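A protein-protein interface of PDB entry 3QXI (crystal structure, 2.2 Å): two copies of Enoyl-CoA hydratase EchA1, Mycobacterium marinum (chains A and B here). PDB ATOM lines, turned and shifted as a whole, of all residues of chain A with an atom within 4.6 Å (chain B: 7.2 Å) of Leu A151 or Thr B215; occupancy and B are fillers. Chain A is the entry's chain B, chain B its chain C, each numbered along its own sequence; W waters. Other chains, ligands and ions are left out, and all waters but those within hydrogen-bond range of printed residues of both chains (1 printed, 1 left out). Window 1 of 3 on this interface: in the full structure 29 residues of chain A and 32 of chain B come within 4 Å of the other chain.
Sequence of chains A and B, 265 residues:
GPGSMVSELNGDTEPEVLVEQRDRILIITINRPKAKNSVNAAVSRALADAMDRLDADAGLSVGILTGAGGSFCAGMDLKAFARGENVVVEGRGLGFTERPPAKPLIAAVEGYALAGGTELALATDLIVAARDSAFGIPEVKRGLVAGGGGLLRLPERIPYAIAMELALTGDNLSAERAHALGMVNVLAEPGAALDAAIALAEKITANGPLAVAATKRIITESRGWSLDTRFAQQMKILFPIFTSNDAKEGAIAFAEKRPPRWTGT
O of Val A140 is in hydrogen-bond range of N of Gly B208 (3.1 Å).
O of Leu A152 is in hydrogen-bond range of NH2 of Arg B223 (3.0 Å).
No position is printed for both chains.
No residue of chain B comes within 4 Å of Gly A150.
Of the printed residues of chain B, Leu A151 touches Thr B215, Ile B218, Ile B219, Ser B222 and Arg B223.
Printed residues of chain B within 4 Å of Leu A152: Ile B218 (3.9 Å), Ser B222 (3.6 Å), Arg B223 (3.0 Å) and Gln B234 (3.5 Å).
Printed residues of chain A within 4 Å of Gly B208: Val A140 (3.1 Å).
Of the printed residues of chain A, Ala B211 touches Val A140 and Val A145.
Of the printed residues of chain A, Thr B215 touches Val A140 (3.4 Å), Val A145 (3.5 Å), Leu A151 (3.9 Å), Ala A167 (3.5 Å) and Leu A168 (3.7 Å).
Printed residues of chain A within 4 Å of Leu B238: Val A145.
Of the printed residues of chain A, Ile B241 touches Val A145 (3.9 Å).
The nearest printed residue of chain A that does not touch Thr B215 is Ala A146 (5.0 Å).
The nearest printed residue of chain B that does not touch Leu A168 is Ile B219 (5.6 Å).
Water W1 lies within hydrogen-bond range of the side-chain hydroxyl of Thr B215 and the backbone NH of Ala A146.
The side-chain hydroxyl of Ser B222 lies within hydrogen-bond range of the guanidinium group of Arg B223, 2.7 Å away.
The backbone carbonyl oxygen of Ile B218 lies within hydrogen-bond range of the side-chain hydroxyl of Ser B222 (2.8 Å).
The backbone carbonyl oxygen of Lys B216 sits at hydrogen-bond distance from the side-chain hydroxyl of Thr B220.
The side-chain hydroxyl of Thr B215 is in hydrogen-bond range of the backbone carbonyl oxygen of Ala B211, at 2.9 Å.
The guanidinium group (NE) of Arg B223 is in hydrogen-bond range of the backbone carbonyl oxygen (O) of Ile B219, 2.9 Å away.
The side-chain hydroxyl (OG) of Ser B222 is in hydrogen-bond range of the backbone carbonyl oxygen (O) of Ile B219 (3.1 Å).
Hydrophobic or aromatic side chains of chain A within 4 Å of the printed part of chain B: Val A140, Val A145, Leu A151, Leu A152, Pro A155, Ala A167 and Leu A168.
Of the 20 printed residues of chain B, 12 touch a printed residue of chain A.
Hydrophobic or aromatic side chains of chain B within 4 Å of the printed part of chain A: Ala B211, Ile B218, Ile B219, Leu B238 and Ile B241.
Among the printed residues, 24 pairs touch across the chains.
Among the printed residues, merely in contact across the chains: Val A145 with Leu B238, Val A145 with Ala B211, Val A140 with Thr B215, Leu A152 with Gln B234, Ala A167 with Ile B219, Val A145 with Thr B215, Ala A167 with Thr B215, Leu A152 with Ser B222, Leu A151 with Ile B218, Leu A168 with Thr B215, Val A140 with Ala B211, Leu A168 with Val B212, Leu A151 with Ile B219, Leu A168 with Lys B216, Pro A155 with Arg B223, Pro A155 with Ile B219, Leu A151 with Thr B215, Val A145 with Ile B241, Leu A152 with Ile B218, Val A140 with Val B212, Leu A151 with Arg B223 and Leu A151 with Ser B222.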
ATOM      1  N   GLU A 119     -21.407  11.031   0.792  1.00  0.00           N
ATOM      2  CA  GLU A 119     -22.134  12.165   1.369  1.00  0.00           C
ATOM      3  C   GLU A 119     -22.848  13.039   0.316  1.00  0.00           C
ATOM      4  O   GLU A 119     -23.969  13.492   0.543  1.00  0.00           O
ATOM      5  CB  GLU A 119     -21.233  12.973   2.283  1.00  0.00           C
ATOM      6  CG  GLU A 119     -20.642  12.115   3.418  1.00  0.00           C
ATOM      7  CD  GLU A 119     -19.819  12.913   4.423  1.00  0.00           C
ATOM      8  OE1 GLU A 119     -18.816  13.553   4.024  1.00  0.00           O
ATOM      9  OE2 GLU A 119     -20.180  12.872   5.626  1.00  0.00           O
ATOM     10  N   ILE A 137     -18.340   4.970   4.097  1.00  0.00           N
ATOM     11  CA  ILE A 137     -17.698   6.054   4.830  1.00  0.00           C
ATOM     12  C   ILE A 137     -16.523   5.462   5.607  1.00  0.00           C
ATOM     13  O   ILE A 137     -16.646   5.148   6.810  1.00  0.00           O
ATOM     14  CB  ILE A 137     -18.694   6.854   5.719  1.00  0.00           C
ATOM     15  CG1 ILE A 137     -19.689   5.890   6.433  1.00  0.00           C
ATOM     16  CG2 ILE A 137     -19.437   7.875   4.853  1.00  0.00           C
ATOM     17  CD1 ILE A 137     -20.663   6.547   7.401  1.00  0.00           C
ATOM     18  N   VAL A 140     -13.202   6.696   9.583  1.00  0.00           N
ATOM     19  CA  VAL A 140     -12.654   6.258  10.870  1.00  0.00           C
ATOM     20  C   VAL A 140     -11.410   5.411  10.722  1.00  0.00           C
ATOM     21  O   VAL A 140     -10.629   5.294  11.661  1.00  0.00           O
ATOM     22  CB  VAL A 140     -13.671   5.439  11.752  1.00  0.00           C
ATOM     23  CG1 VAL A 140     -14.766   6.330  12.295  1.00  0.00           C
ATOM     24  CG2 VAL A 140     -14.231   4.219  10.982  1.00  0.00           C
ATOM     25  N   VAL A 145     -13.555  11.661  10.779  1.00  0.00           N
ATOM     26  CA  VAL A 145     -15.007  11.469  10.940  1.00  0.00           C
ATOM     27  C   VAL A 145     -15.716  12.098   9.751  1.00  0.00           C
ATOM     28  O   VAL A 145     -15.340  13.194   9.268  1.00  0.00           O
ATOM     29  CB  VAL A 145     -15.500  11.993  12.286  1.00  0.00           C
ATOM     30  CG1 VAL A 145     -17.015  11.825  12.444  1.00  0.00           C
ATOM     31  CG2 VAL A 145     -14.802  11.245  13.440  1.00  0.00           C
ATOM     32  N   ALA A 146     -16.700  11.391   9.227  1.00  0.00           N
ATOM     33  CA  ALA A 146     -17.427  11.929   8.109  1.00  0.00           C
ATOM     34  C   ALA A 146     -18.206  13.149   8.600  1.00  0.00           C
ATOM     35  O   ALA A 146     -19.093  13.016   9.449  1.00  0.00           O
ATOM     36  CB  ALA A 146     -18.353  10.880   7.552  1.00  0.00           C
ATOM     37  N   GLY A 149     -22.363  15.086   6.373  1.00  0.00           N
ATOM     38  CA  GLY A 149     -23.749  14.663   6.608  1.00  0.00           C
ATOM     39  C   GLY A 149     -24.059  13.188   6.420  1.00  0.00           C
ATOM     40  O   GLY A 149     -25.208  12.734   6.655  1.00  0.00           O
ATOM     41  N   GLY A 150     -23.052  12.427   5.992  1.00  0.00           N
ATOM     42  CA  GLY A 150     -23.145  10.966   5.954  1.00  0.00           C
ATOM     43  C   GLY A 150     -23.626  10.373   7.255  1.00  0.00           C
ATOM     44  O   GLY A 150     -24.438   9.459   7.246  1.00  0.00           O
ATOM     45  N   LEU A 151     -23.156  10.901   8.383  1.00  0.00           N
ATOM     46  CA  LEU A 151     -23.570  10.349   9.674  1.00  0.00           C
ATOM     47  C   LEU A 151     -24.974  10.831  10.051  1.00  0.00           C
ATOM     48  O   LEU A 151     -25.613  10.261  10.940  1.00  0.00           O
ATOM     49  CB  LEU A 151     -22.585  10.723  10.784  1.00  0.00           C
ATOM     50  CG  LEU A 151     -21.138  10.267  10.596  1.00  0.00           C
ATOM     51  CD1 LEU A 151     -20.281  10.592  11.809  1.00  0.00           C
ATOM     52  CD2 LEU A 151     -21.032   8.735  10.265  1.00  0.00           C
ATOM     53  N   LEU A 152     -25.447  11.881   9.388  1.00  0.00           N
ATOM     54  CA  LEU A 152     -26.790  12.377   9.679  1.00  0.00           C
ATOM     55  C   LEU A 152     -27.809  11.681   8.780  1.00  0.00           C
ATOM     56  O   LEU A 152     -28.930  11.379   9.214  1.00  0.00           O
ATOM     57  CB  LEU A 152     -26.868  13.910   9.505  1.00  0.00           C
ATOM     58  CG  LEU A 152     -25.770  14.756  10.143  1.00  0.00           C
ATOM     59  CD1 LEU A 152     -25.910  16.165   9.731  1.00  0.00           C
ATOM     60  CD2 LEU A 152     -25.788  14.650  11.641  1.00  0.00           C
ATOM     61  N   ARG A 153     -27.416  11.442   7.530  1.00  0.00           N
ATOM     62  CA  ARG A 153     -28.332  10.903   6.523  1.00  0.00           C
ATOM     63  C   ARG A 153     -28.294   9.383   6.388  1.00  0.00           C
ATOM     64  O   ARG A 153     -29.360   8.755   6.238  1.00  0.00           O
ATOM     65  CB  ARG A 153     -28.095  11.561   5.162  1.00  0.00           C
ATOM     66  CG  ARG A 153     -28.447  13.060   5.167  1.00  0.00           C
ATOM     67  CD  ARG A 153     -28.110  13.767   3.829  1.00  0.00           C
ATOM     68  NE  ARG A 153     -28.692  15.119   3.778  1.00  0.00           N
ATOM     69  CZ  ARG A 153     -27.986  16.251   3.693  1.00  0.00           C
ATOM     70  NH1 ARG A 153     -26.648  16.238   3.606  1.00  0.00           N
ATOM     71  NH2 ARG A 153     -28.625  17.410   3.661  1.00  0.00           N
ATOM     72  N   PRO A 155     -28.233   6.870   8.506  1.00  0.00           N
ATOM     73  CA  PRO A 155     -29.200   6.173   9.366  1.00  0.00           C
ATOM     74  C   PRO A 155     -30.662   6.495   9.037  1.00  0.00           C
ATOM     75  O   PRO A 155     -31.586   5.844   9.560  1.00  0.00           O
ATOM     76  CB  PRO A 155     -28.865   6.684  10.780  1.00  0.00           C
ATOM     77  CG  PRO A 155     -27.611   7.383  10.694  1.00  0.00           C
ATOM     78  CD  PRO A 155     -27.490   7.888   9.271  1.00  0.00           C
ATOM     79  N   ALA A 167     -20.564   2.855   9.551  1.00  0.00           N
ATOM     80  CA  ALA A 167     -19.876   4.040  10.098  1.00  0.00           C
ATOM     81  C   ALA A 167     -18.692   3.686  11.021  1.00  0.00           C
ATOM     82  O   ALA A 167     -17.622   4.301  10.952  1.00  0.00           O
ATOM     83  CB  ALA A 167     -20.849   4.933  10.818  1.00  0.00           C
ATOM     84  N   LEU A 168     -18.889   2.690  11.861  1.00  0.00           N
ATOM     85  CA  LEU A 168     -17.870   2.292  12.830  1.00  0.00           C
ATOM     86  C   LEU A 168     -16.758   1.388  12.240  1.00  0.00           C
ATOM     87  O   LEU A 168     -15.583   1.463  12.680  1.00  0.00           O
ATOM     88  CB  LEU A 168     -18.535   1.612  14.029  1.00  0.00           C
ATOM     89  CG  LEU A 168     -19.630   2.372  14.818  1.00  0.00           C
ATOM     90  CD1 LEU A 168     -19.967   1.559  16.030  1.00  0.00           C
ATOM     91  CD2 LEU A 168     -19.275   3.860  15.241  1.00  0.00           C
ATOM     92  N   GLY B 208      -9.525   4.245  14.379  1.00  0.00           N
ATOM     93  CA  GLY B 208      -9.175   5.347  15.298  1.00  0.00           C
ATOM     94  C   GLY B 208     -10.203   5.600  16.398  1.00  0.00           C
ATOM     95  O   GLY B 208     -11.331   5.984  16.098  1.00  0.00           O
ATOM     96  N   PRO B 209      -9.804   5.398  17.675  1.00  0.00           N
ATOM     97  CA  PRO B 209     -10.702   5.376  18.827  1.00  0.00           C
ATOM     98  C   PRO B 209     -11.475   6.682  19.109  1.00  0.00           C
ATOM     99  O   PRO B 209     -12.615   6.604  19.556  1.00  0.00           O
ATOM    100  CB  PRO B 209      -9.767   5.016  20.012  1.00  0.00           C
ATOM    101  CG  PRO B 209      -8.331   5.275  19.467  1.00  0.00           C
ATOM    102  CD  PRO B 209      -8.448   4.930  18.036  1.00  0.00           C
ATOM    103  N   LEU B 210     -10.847   7.839  18.899  1.00  0.00           N
ATOM    104  CA  LEU B 210     -11.544   9.136  19.021  1.00  0.00           C
ATOM    105  C   LEU B 210     -12.555   9.281  17.922  1.00  0.00           C
ATOM    106  O   LEU B 210     -13.658   9.731  18.165  1.00  0.00           O
ATOM    107  CB  LEU B 210     -10.595  10.331  18.907  1.00  0.00           C
ATOM    108  CG  LEU B 210      -9.759  10.761  20.097  1.00  0.00           C
ATOM    109  CD1 LEU B 210      -8.747  11.749  19.587  1.00  0.00           C
ATOM    110  CD2 LEU B 210     -10.630  11.350  21.272  1.00  0.00           C
ATOM    111  N   ALA B 211     -12.147   8.923  16.710  1.00  0.00           N
ATOM    112  CA  ALA B 211     -13.021   8.977  15.520  1.00  0.00           C
ATOM    113  C   ALA B 211     -14.248   8.042  15.641  1.00  0.00           C
ATOM    114  O   ALA B 211     -15.372   8.425  15.309  1.00  0.00           O
ATOM    115  CB  ALA B 211     -12.214   8.670  14.265  1.00  0.00           C
ATOM    116  N   VAL B 212     -14.011   6.831  16.137  1.00  0.00           N
ATOM    117  CA  VAL B 212     -15.076   5.829  16.370  1.00  0.00           C
ATOM    118  C   VAL B 212     -16.060   6.322  17.421  1.00  0.00           C
ATOM    119  O   VAL B 212     -17.286   6.321  17.198  1.00  0.00           O
ATOM    120  CB  VAL B 212     -14.452   4.450  16.728  1.00  0.00           C
ATOM    121  CG1 VAL B 212     -15.504   3.485  17.362  1.00  0.00           C
ATOM    122  CG2 VAL B 212     -13.812   3.817  15.474  1.00  0.00           C
ATOM    123  N   ALA B 213     -15.521   6.827  18.531  1.00  0.00           N
ATOM    124  CA  ALA B 213     -16.342   7.363  19.594  1.00  0.00           C
ATOM    125  C   ALA B 213     -17.189   8.535  19.131  1.00  0.00           C
ATOM    126  O   ALA B 213     -18.387   8.588  19.458  1.00  0.00           O
ATOM    127  CB  ALA B 213     -15.500   7.754  20.819  1.00  0.00           C
ATOM    128  N   ALA B 214     -16.588   9.469  18.382  1.00  0.00           N
ATOM    129  CA  ALA B 214     -17.358  10.610  17.872  1.00  0.00           C
ATOM    130  C   ALA B 214     -18.384  10.176  16.824  1.00  0.00           C
ATOM    131  O   ALA B 214     -19.481  10.714  16.769  1.00  0.00           O
ATOM    132  CB  ALA B 214     -16.441  11.705  17.284  1.00  0.00           C
ATOM    133  N   THR B 215     -18.005   9.233  15.965  1.00  0.00           N
ATOM    134  CA  THR B 215     -18.931   8.684  14.990  1.00  0.00           C
ATOM    135  C   THR B 215     -20.220   8.120  15.644  1.00  0.00           C
ATOM    136  O   THR B 215     -21.348   8.479  15.230  1.00  0.00           O
ATOM    137  CB  THR B 215     -18.240   7.682  14.087  1.00  0.00           C
ATOM    138  OG1 THR B 215     -17.337   8.400  13.232  1.00  0.00           O
ATOM    139  CG2 THR B 215     -19.247   6.966  13.218  1.00  0.00           C
ATOM    140  N   LYS B 216     -20.057   7.278  16.664  1.00  0.00           N
ATOM    141  CA  LYS B 216     -21.193   6.685  17.370  1.00  0.00           C
ATOM    142  C   LYS B 216     -22.041   7.792  17.995  1.00  0.00           C
ATOM    143  O   LYS B 216     -23.266   7.809  17.874  1.00  0.00           O
ATOM    144  CB  LYS B 216     -20.744   5.690  18.451  1.00  0.00           C
ATOM    145  CG  LYS B 216     -21.854   5.324  19.435  1.00  0.00           C
ATOM    146  CD  LYS B 216     -21.449   4.150  20.367  1.00  0.00           C
ATOM    147  CE  LYS B 216     -22.439   4.056  21.530  1.00  0.00           C
ATOM    148  NZ  LYS B 216     -22.303   2.778  22.318  1.00  0.00           N
ATOM    149  N   ARG B 217     -21.350   8.723  18.644  1.00  0.00           N
ATOM    150  CA  ARG B 217     -21.973   9.871  19.281  1.00  0.00           C
ATOM    151  C   ARG B 217     -22.870  10.652  18.321  1.00  0.00           C
ATOM    152  O   ARG B 217     -24.045  10.976  18.631  1.00  0.00           O
ATOM    153  CB  ARG B 217     -20.877  10.777  19.866  1.00  0.00           C
ATOM    154  CG  ARG B 217     -21.478  11.870  20.648  1.00  0.00           C
ATOM    155  CD  ARG B 217     -20.564  12.685  21.523  1.00  0.00           C
ATOM    156  NE  ARG B 217     -21.437  13.662  22.186  1.00  0.00           N
ATOM    157  CZ  ARG B 217     -21.050  14.823  22.696  1.00  0.00           C
ATOM    158  NH1 ARG B 217     -19.776  15.204  22.648  1.00  0.00           N
ATOM    159  NH2 ARG B 217     -21.956  15.603  23.266  1.00  0.00           N
ATOM    160  N   ILE B 218     -22.336  10.958  17.143  1.00  0.00           N
ATOM    161  CA  ILE B 218     -23.096  11.745  16.163  1.00  0.00           C
ATOM    162  C   ILE B 218     -24.301  10.980  15.650  1.00  0.00           C
ATOM    163  O   ILE B 218     -25.399  11.542  15.545  1.00  0.00           O
ATOM    164  CB  ILE B 218     -22.226  12.234  15.011  1.00  0.00           C
ATOM    165  CG1 ILE B 218     -21.270  13.317  15.531  1.00  0.00           C
ATOM    166  CG2 ILE B 218     -23.087  12.782  13.817  1.00  0.00           C
ATOM    167  CD1 ILE B 218     -20.069  13.585  14.583  1.00  0.00           C
ATOM    168  N   ILE B 219     -24.111   9.705  15.329  1.00  0.00           N
ATOM    169  CA  ILE B 219     -25.229   8.915  14.846  1.00  0.00           C
ATOM    170  C   ILE B 219     -26.378   8.847  15.868  1.00  0.00           C
ATOM    171  O   ILE B 219     -27.568   9.029  15.513  1.00  0.00           O
ATOM    172  CB  ILE B 219     -24.805   7.517  14.396  1.00  0.00           C
ATOM    173  CG1 ILE B 219     -23.965   7.659  13.118  1.00  0.00           C
ATOM    174  CG2 ILE B 219     -26.031   6.672  14.162  1.00  0.00           C
ATOM    175  CD1 ILE B 219     -23.443   6.430  12.563  1.00  0.00           C
ATOM    176  N   THR B 220     -25.997   8.585  17.114  1.00  0.00           N
ATOM    177  CA  THR B 220     -26.904   8.481  18.240  1.00  0.00           C
ATOM    178  C   THR B 220     -27.626   9.826  18.515  1.00  0.00           C
ATOM    179  O   THR B 220     -28.871   9.887  18.478  1.00  0.00           O
ATOM    180  CB  THR B 220     -26.084   8.039  19.471  1.00  0.00           C
ATOM    181  OG1 THR B 220     -25.602   6.711  19.217  1.00  0.00           O
ATOM    182  CG2 THR B 220     -26.961   8.031  20.721  1.00  0.00           C
ATOM    183  N   GLU B 221     -26.865  10.901  18.744  1.00  0.00           N
ATOM    184  CA  GLU B 221     -27.492  12.183  19.097  1.00  0.00           C
ATOM    185  C   GLU B 221     -28.248  12.849  17.968  1.00  0.00           C
ATOM    186  O   GLU B 221     -29.274  13.497  18.204  1.00  0.00           O
ATOM    187  CB  GLU B 221     -26.527  13.116  19.786  1.00  0.00           C
ATOM    188  CG  GLU B 221     -26.063  12.569  21.147  1.00  0.00           C
ATOM    189  CD  GLU B 221     -24.841  13.270  21.654  1.00  0.00           C
ATOM    190  OE1 GLU B 221     -24.677  14.462  21.379  1.00  0.00           O
ATOM    191  OE2 GLU B 221     -24.027  12.637  22.350  1.00  0.00           O
ATOM    192  N   SER B 222     -27.801  12.627  16.732  1.00  0.00           N
ATOM    193  CA  SER B 222     -28.384  13.331  15.581  1.00  0.00           C
ATOM    194  C   SER B 222     -29.880  13.084  15.363  1.00  0.00           C
ATOM    195  O   SER B 222     -30.587  13.917  14.778  1.00  0.00           O
ATOM    196  CB  SER B 222     -27.594  13.046  14.313  1.00  0.00           C
ATOM    197  OG  SER B 222     -27.758  11.716  13.958  1.00  0.00           O
ATOM    198  N   ARG B 223     -30.346  11.937  15.840  1.00  0.00           N
ATOM    199  CA  ARG B 223     -31.758  11.566  15.818  1.00  0.00           C
ATOM    200  C   ARG B 223     -32.600  12.689  16.435  1.00  0.00           C
ATOM    201  O   ARG B 223     -33.699  12.974  15.938  1.00  0.00           O
ATOM    202  CB  ARG B 223     -31.992  10.217  16.552  1.00  0.00           C
ATOM    203  CG  ARG B 223     -30.917   9.072  16.262  1.00  0.00           C
ATOM    204  CD  ARG B 223     -30.838   8.616  14.778  1.00  0.00           C
ATOM    205  NE  ARG B 223     -29.985   9.511  13.992  1.00  0.00           N
ATOM    206  CZ  ARG B 223     -30.220   9.857  12.725  1.00  0.00           C
ATOM    207  NH1 ARG B 223     -31.283   9.357  12.095  1.00  0.00           N
ATOM    208  NH2 ARG B 223     -29.393  10.703  12.088  1.00  0.00           N
ATOM    209  N   GLN B 234     -23.213  18.717  15.110  1.00  0.00           N
ATOM    210  CA  GLN B 234     -22.170  17.796  14.648  1.00  0.00           C
ATOM    211  C   GLN B 234     -20.765  18.423  14.752  1.00  0.00           C
ATOM    212  O   GLN B 234     -19.862  17.827  15.346  1.00  0.00           O
ATOM    213  CB  GLN B 234     -22.475  17.344  13.220  1.00  0.00           C
ATOM    214  CG  GLN B 234     -21.439  16.453  12.558  1.00  0.00           C
ATOM    215  CD  GLN B 234     -21.907  15.971  11.185  1.00  0.00           C
ATOM    216  OE1 GLN B 234     -22.379  14.851  11.048  1.00  0.00           O
ATOM    217  NE2 GLN B 234     -21.816  16.837  10.184  1.00  0.00           N
ATOM    218  N   ILE B 237     -18.920  18.177  17.984  1.00  0.00           N
ATOM    219  CA  ILE B 237     -18.268  16.854  18.155  1.00  0.00           C
ATOM    220  C   ILE B 237     -17.056  16.588  17.230  1.00  0.00           C
ATOM    221  O   ILE B 237     -16.053  15.978  17.646  1.00  0.00           O
ATOM    222  CB  ILE B 237     -19.323  15.712  18.011  1.00  0.00           C
ATOM    223  CG1 ILE B 237     -20.502  15.997  18.946  1.00  0.00           C
ATOM    224  CG2 ILE B 237     -18.686  14.341  18.274  1.00  0.00           C
ATOM    225  CD1 ILE B 237     -21.726  15.167  18.683  1.00  0.00           C
ATOM    226  N   LEU B 238     -17.143  17.055  15.983  1.00  0.00           N
ATOM    227  CA  LEU B 238     -16.024  16.932  15.055  1.00  0.00           C
ATOM    228  C   LEU B 238     -14.802  17.759  15.472  1.00  0.00           C
ATOM    229  O   LEU B 238     -13.668  17.432  15.121  1.00  0.00           O
ATOM    230  CB  LEU B 238     -16.423  17.349  13.631  1.00  0.00           C
ATOM    231  CG  LEU B 238     -17.598  16.683  12.900  1.00  0.00           C
ATOM    232  CD1 LEU B 238     -17.860  17.381  11.538  1.00  0.00           C
ATOM    233  CD2 LEU B 238     -17.403  15.199  12.706  1.00  0.00           C
ATOM    234  N   ILE B 241     -11.462  16.411  16.409  1.00  0.00           N
ATOM    235  CA  ILE B 241     -10.930  15.423  15.471  1.00  0.00           C
ATOM    236  C   ILE B 241      -9.930  16.064  14.499  1.00  0.00           C
ATOM    237  O   ILE B 241      -8.933  15.457  14.148  1.00  0.00           O
ATOM    238  CB  ILE B 241     -12.031  14.677  14.667  1.00  0.00           C
ATOM    239  CG1 ILE B 241     -13.084  14.039  15.591  1.00  0.00           C
ATOM    240  CG2 ILE B 241     -11.390  13.631  13.768  1.00  0.00           C
ATOM    241  CD1 ILE B 241     -12.532  13.251  16.841  1.00  0.00           C
HETATM  242  O   HOH W   1     -17.308   8.833  10.427  1.00  0.00           O
